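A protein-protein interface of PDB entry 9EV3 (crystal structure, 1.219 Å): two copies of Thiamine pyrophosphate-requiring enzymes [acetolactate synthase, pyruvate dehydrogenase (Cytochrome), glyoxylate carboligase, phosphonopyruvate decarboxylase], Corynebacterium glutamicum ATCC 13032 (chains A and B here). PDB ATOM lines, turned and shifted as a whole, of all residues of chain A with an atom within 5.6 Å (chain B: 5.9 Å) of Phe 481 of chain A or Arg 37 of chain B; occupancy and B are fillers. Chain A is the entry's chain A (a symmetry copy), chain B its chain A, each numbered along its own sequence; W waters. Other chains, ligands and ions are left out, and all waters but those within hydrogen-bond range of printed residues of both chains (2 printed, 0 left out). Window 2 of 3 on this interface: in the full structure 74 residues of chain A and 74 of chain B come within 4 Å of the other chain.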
ATOM      1  N   MET A 473     -31.118 -17.937  -5.474  1.00  0.00           N
ATOM      2  CA  MET A 473     -30.529 -16.596  -5.489  1.00  0.00           C
ATOM      3  C   MET A 473     -31.595 -15.524  -5.667  1.00  0.00           C
ATOM      4  O   MET A 473     -31.469 -14.433  -5.105  1.00  0.00           O
ATOM      5  CB  MET A 473     -29.485 -16.479  -6.589  1.00  0.00           C
ATOM      6  CG  MET A 473     -28.242 -17.258  -6.271  1.00  0.00           C
ATOM      7  SD  MET A 473     -27.005 -17.055  -7.564  1.00  0.00           S
ATOM      8  CE  MET A 473     -25.700 -18.145  -6.898  1.00  0.00           C
ATOM      9  N   PRO A 479     -27.742 -10.776  -6.428  1.00  0.00           N
ATOM     10  CA  PRO A 479     -27.543 -10.721  -7.889  1.00  0.00           C
ATOM     11  C   PRO A 479     -27.184 -12.069  -8.485  1.00  0.00           C
ATOM     12  O   PRO A 479     -26.419 -12.830  -7.889  1.00  0.00           O
ATOM     13  CB  PRO A 479     -26.391  -9.730  -8.051  1.00  0.00           C
ATOM     14  CG  PRO A 479     -26.516  -8.828  -6.861  1.00  0.00           C
ATOM     15  CD  PRO A 479     -26.993  -9.710  -5.735  1.00  0.00           C
ATOM     16  N   GLU A 480     -27.800 -12.408  -9.619  1.00  0.00           N
ATOM     17  CA  GLU A 480     -27.555 -13.692 -10.263  1.00  0.00           C
ATOM     18  C   GLU A 480     -26.102 -13.818 -10.669  1.00  0.00           C
ATOM     19  O   GLU A 480     -25.579 -12.940 -11.358  1.00  0.00           O
ATOM     20  CB  GLU A 480     -28.452 -13.839 -11.498  1.00  0.00           C
ATOM     21  CG  GLU A 480     -28.259 -15.161 -12.222  1.00  0.00           C
ATOM     22  CD  GLU A 480     -28.692 -15.097 -13.671  1.00  0.00           C
ATOM     23  OE1 GLU A 480     -29.706 -14.416 -13.959  1.00  0.00           O
ATOM     24  OE2 GLU A 480     -27.996 -15.692 -14.523  1.00  0.00           O
ATOM     25  N   PHE A 481     -25.444 -14.900 -10.231  1.00  0.00           N
ATOM     26  CA  PHE A 481     -24.049 -15.096 -10.582  1.00  0.00           C
ATOM     27  C   PHE A 481     -23.682 -16.544 -10.518  1.00  0.00           C
ATOM     28  O   PHE A 481     -24.049 -17.225  -9.569  1.00  0.00           O
ATOM     29  CB  PHE A 481     -23.166 -14.294  -9.625  1.00  0.00           C
ATOM     30  CG  PHE A 481     -21.692 -14.319  -9.946  1.00  0.00           C
ATOM     31  CD1 PHE A 481     -21.155 -13.452 -10.881  1.00  0.00           C
ATOM     32  CD2 PHE A 481     -20.843 -15.198  -9.302  1.00  0.00           C
ATOM     33  CE1 PHE A 481     -19.791 -13.457 -11.152  1.00  0.00           C
ATOM     34  CE2 PHE A 481     -19.477 -15.193  -9.562  1.00  0.00           C
ATOM     35  CZ  PHE A 481     -18.959 -14.318 -10.480  1.00  0.00           C
ATOM     36  N   GLY A 482     -23.008 -17.022 -11.555  1.00  0.00           N
ATOM     37  CA  GLY A 482     -22.488 -18.374 -11.558  1.00  0.00           C
ATOM     38  C   GLY A 482     -23.430 -19.480 -11.941  1.00  0.00           C
ATOM     39  O   GLY A 482     -23.031 -20.640 -11.907  1.00  0.00           O
ATOM     40  N   THR A 483     -24.677 -19.150 -12.325  1.00  0.00           N
ATOM     41  CA  THR A 483     -25.650 -20.205 -12.635  1.00  0.00           C
ATOM     42  C   THR A 483     -25.848 -20.454 -14.115  1.00  0.00           C
ATOM     43  O   THR A 483     -26.113 -21.594 -14.530  1.00  0.00           O
ATOM     44  CB  THR A 483     -27.018 -19.865 -12.012  1.00  0.00           C
ATOM     45  OG1 THR A 483     -27.503 -18.611 -12.517  1.00  0.00           O
ATOM     46  CG2 THR A 483     -26.980 -19.833 -10.500  1.00  0.00           C
ATOM     47  N   VAL B  25     -21.398 -23.560  -8.254  1.00  0.00           N
ATOM     48  CA  VAL B  25     -22.231 -22.907  -7.263  1.00  0.00           C
ATOM     49  C   VAL B  25     -23.451 -23.755  -6.870  1.00  0.00           C
ATOM     50  O   VAL B  25     -23.939 -24.530  -7.666  1.00  0.00           O
ATOM     51  CB  VAL B  25     -22.647 -21.475  -7.698  1.00  0.00           C
ATOM     52  CG1 VAL B  25     -23.796 -21.521  -8.688  1.00  0.00           C
ATOM     53  CG2 VAL B  25     -23.017 -20.624  -6.489  1.00  0.00           C
ATOM     54  N   ILE B  32     -21.017 -17.038  -0.309  1.00  0.00           N
ATOM     55  CA  ILE B  32     -19.592 -16.975  -0.630  1.00  0.00           C
ATOM     56  C   ILE B  32     -19.428 -16.554  -2.090  1.00  0.00           C
ATOM     57  O   ILE B  32     -18.553 -15.728  -2.398  1.00  0.00           O
ATOM     58  CB  ILE B  32     -18.963 -18.328  -0.305  1.00  0.00           C
ATOM     59  CG1 ILE B  32     -19.041 -18.524   1.218  1.00  0.00           C
ATOM     60  CG2 ILE B  32     -17.530 -18.347  -0.809  1.00  0.00           C
ATOM     61  CD1 ILE B  32     -18.492 -19.871   1.719  1.00  0.00           C
ATOM     62  N   VAL B  33     -20.268 -17.100  -3.005  1.00  0.00           N
ATOM     63  CA  VAL B  33     -20.144 -16.717  -4.415  1.00  0.00           C
ATOM     64  C   VAL B  33     -20.541 -15.249  -4.603  1.00  0.00           C
ATOM     65  O   VAL B  33     -19.924 -14.573  -5.447  1.00  0.00           O
ATOM     66  CB  VAL B  33     -20.941 -17.688  -5.293  1.00  0.00           C
ATOM     67  CG1 VAL B  33     -21.074 -17.187  -6.728  1.00  0.00           C
ATOM     68  CG2 VAL B  33     -20.220 -19.039  -5.261  1.00  0.00           C
ATOM     69  N   ASP B  34     -21.483 -14.730  -3.822  1.00  0.00           N
ATOM     70  CA  ASP B  34     -21.829 -13.304  -3.915  1.00  0.00           C
ATOM     71  C   ASP B  34     -20.609 -12.452  -3.535  1.00  0.00           C
ATOM     72  O   ASP B  34     -20.363 -11.389  -4.154  1.00  0.00           O
ATOM     73  CB  ASP B  34     -22.997 -12.981  -2.982  1.00  0.00           C
ATOM     74  CG  ASP B  34     -23.761 -11.742  -3.391  1.00  0.00           C
ATOM     75  OD1 ASP B  34     -23.702 -11.378  -4.583  1.00  0.00           O
ATOM     76  OD2 ASP B  34     -24.466 -11.193  -2.548  1.00  0.00           O
ATOM     77  N   ALA B  35     -19.858 -12.893  -2.503  1.00  0.00           N
ATOM     78  CA  ALA B  35     -18.668 -12.146  -2.116  1.00  0.00           C
ATOM     79  C   ALA B  35     -17.604 -12.246  -3.191  1.00  0.00           C
ATOM     80  O   ALA B  35     -16.920 -11.248  -3.473  1.00  0.00           O
ATOM     81  CB  ALA B  35     -18.132 -12.656  -0.782  1.00  0.00           C
ATOM     82  N   VAL B  36     -17.468 -13.412  -3.853  1.00  0.00           N
ATOM     83  CA  VAL B  36     -16.513 -13.504  -4.950  1.00  0.00           C
ATOM     84  C   VAL B  36     -16.856 -12.524  -6.074  1.00  0.00           C
ATOM     85  O   VAL B  36     -15.973 -11.847  -6.612  1.00  0.00           O
ATOM     86  CB  VAL B  36     -16.504 -14.943  -5.491  1.00  0.00           C
ATOM     87  CG1 VAL B  36     -15.657 -15.031  -6.770  1.00  0.00           C
ATOM     88  CG2 VAL B  36     -15.957 -15.895  -4.411  1.00  0.00           C
ATOM     89  N   ARG B  37     -18.161 -12.415  -6.388  1.00  0.00           N
ATOM     90  CA  ARG B  37     -18.602 -11.515  -7.484  1.00  0.00           C
ATOM     91  C   ARG B  37     -18.147 -10.090  -7.233  1.00  0.00           C
ATOM     92  O   ARG B  37     -17.754  -9.381  -8.179  1.00  0.00           O
ATOM     93  CB  ARG B  37     -20.126 -11.554  -7.558  1.00  0.00           C
ATOM     94  CG  ARG B  37     -20.739 -10.558  -8.545  1.00  0.00           C
ATOM     95  CD  ARG B  37     -22.267 -10.541  -8.407  1.00  0.00           C
ATOM     96  NE  ARG B  37     -22.719 -10.140  -7.071  1.00  0.00           N
ATOM     97  CZ  ARG B  37     -22.931  -8.879  -6.692  1.00  0.00           C
ATOM     98  NH1 ARG B  37     -22.723  -7.879  -7.538  1.00  0.00           N
ATOM     99  NH2 ARG B  37     -23.341  -8.610  -5.456  1.00  0.00           N
ATOM    100  N   GLN B  38     -18.205  -9.673  -5.970  1.00  0.00           N
ATOM    101  CA  GLN B  38     -17.830  -8.312  -5.574  1.00  0.00           C
ATOM    102  C   GLN B  38     -16.344  -8.088  -5.387  1.00  0.00           C
ATOM    103  O   GLN B  38     -15.936  -6.947  -5.146  1.00  0.00           O
ATOM    104  CB  GLN B  38     -18.533  -7.949  -4.296  1.00  0.00           C
ATOM    105  CG  GLN B  38     -20.046  -7.939  -4.463  1.00  0.00           C
ATOM    106  CD  GLN B  38     -20.693  -7.876  -3.101  1.00  0.00           C
ATOM    107  OE1 GLN B  38     -20.254  -8.518  -2.133  1.00  0.00           O
ATOM    108  NE2 GLN B  38     -21.763  -7.115  -2.997  1.00  0.00           N
ATOM    109  N   SER B  39     -15.526  -9.130  -5.479  1.00  0.00           N
ATOM    110  CA  SER B  39     -14.086  -9.067  -5.319  1.00  0.00           C
ATOM    111  C   SER B  39     -13.382  -9.103  -6.666  1.00  0.00           C
ATOM    112  O   SER B  39     -14.035  -9.232  -7.730  1.00  0.00           O
ATOM    113  CB  SER B  39     -13.646 -10.311  -4.513  1.00  0.00           C
ATOM    114  OG  SER B  39     -13.554 -11.455  -5.352  1.00  0.00           O
ATOM    115  N   ILE B  41     -11.404 -11.653  -7.353  1.00  0.00           N
ATOM    116  CA  ILE B  41     -11.168 -13.092  -7.618  1.00  0.00           C
ATOM    117  C   ILE B  41     -12.131 -13.567  -8.686  1.00  0.00           C
ATOM    118  O   ILE B  41     -13.333 -13.247  -8.659  1.00  0.00           O
ATOM    119  CB  ILE B  41     -11.366 -13.861  -6.294  1.00  0.00           C
ATOM    120  CG1 ILE B  41     -10.319 -13.440  -5.261  1.00  0.00           C
ATOM    121  CG2 ILE B  41     -11.268 -15.414  -6.524  1.00  0.00           C
ATOM    122  CD1 ILE B  41     -10.497 -14.189  -3.885  1.00  0.00           C
ATOM    123  N   TRP B  43     -14.327 -16.477 -10.521  1.00  0.00           N
ATOM    124  CA  TRP B  43     -14.957 -17.766 -10.278  1.00  0.00           C
ATOM    125  C   TRP B  43     -14.792 -18.604 -11.534  1.00  0.00           C
ATOM    126  O   TRP B  43     -15.238 -18.164 -12.611  1.00  0.00           O
ATOM    127  CB  TRP B  43     -16.434 -17.522  -9.982  1.00  0.00           C
ATOM    128  CG  TRP B  43     -17.194 -18.740  -9.639  1.00  0.00           C
ATOM    129  CD1 TRP B  43     -18.150 -19.344 -10.416  1.00  0.00           C
ATOM    130  CD2 TRP B  43     -17.128 -19.484  -8.418  1.00  0.00           C
ATOM    131  NE1 TRP B  43     -18.610 -20.480  -9.800  1.00  0.00           N
ATOM    132  CE2 TRP B  43     -18.021 -20.576  -8.548  1.00  0.00           C
ATOM    133  CE3 TRP B  43     -16.483 -19.286  -7.182  1.00  0.00           C
ATOM    134  CZ2 TRP B  43     -18.182 -21.525  -7.538  1.00  0.00           C
ATOM    135  CZ3 TRP B  43     -16.652 -20.232  -6.173  1.00  0.00           C
ATOM    136  CH2 TRP B  43     -17.512 -21.334  -6.362  1.00  0.00           C
HETATM  137  O   HOH W   1     -24.084 -12.823  -6.822  1.00  0.00           O
HETATM  138  O   HOH W   2     -20.845 -22.124 -10.675  1.00  0.00           O
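Among the printed residues, pairs that only touch across the chains: Phe 481 of chain A with Val 33 of chain B (3.3 Å), Gly 482 of chain A with Val 25 of chain B (3.4 Å), Pro 479 of chain A with Arg 37 of chain B (3.5 Å), Met 473 of chain A with Val 25 of chain B (3.7 Å), Phe 481 of chain A with Arg 37 of chain B (3.7 Å), Phe 481 of chain A with Trp 43 of chain B (3.9 Å) and Pro 479 of chain A with Asp 34 of chain B (3.9 Å).
Water W1 lies within hydrogen-bond range of O of Pro 479 of chain A (2.6 Å), OD1 of Asp 34 of chain B (2.7 Å) and NE of Arg 37 of chain B (3.0 Å).
Water W2 lies within hydrogen-bond range of N of Val 25 of chain B (2.9 Å), NE1 of Trp 43 of chain B (2.9 Å) and O of Gly 482 of chain A (2.9 Å).
Arg 37 of chain B touches two residues of chain A.
Of the printed residues of chain A, Val 33 of chain B touches Phe 481 (3.3 Å).
Of the printed residues of chain B, Met 473 of chain A touches Val 25.
Gln 38 of chain B touches none of the printed residues of chain A.
The nearest printed residue of chain B that does not touch Phe 481 of chain A is Val 25 of chain B (4.4 Å).
The side-chain carboxylate (OD1) of Asp 34 of chain B is in salt-bridge range of the guanidinium group (NH2) of Arg 37 of chain B (2.9 Å).
NH2 of Arg 37 of chain B sits close to NE2 of Gln 38 of chain B (3.3 Å).
The side-chain sulfur of Met 473 of chain A sits at hydrogen-bond distance from the backbone NH of Phe 481 of chain A, at 3.8 Å.
Of the 6 printed residues of chain A, 4 touch a printed residue of chain B.
Printed residues of chain A that touch a printed residue of chain B: Met 473, Pro 479, Phe 481 and Gly 482.
Of the 11 printed residues of chain B, 5 touch a printed residue of chain A.
Hydrophobic or aromatic side chains of chain B that line the printed part of chain A: Val 25, Val 33 and Trp 43.
No position is printed for both chains.
Of the 7 pairs that touch across the chains among the printed residues, none has its exchanged pair printed and touching as well.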
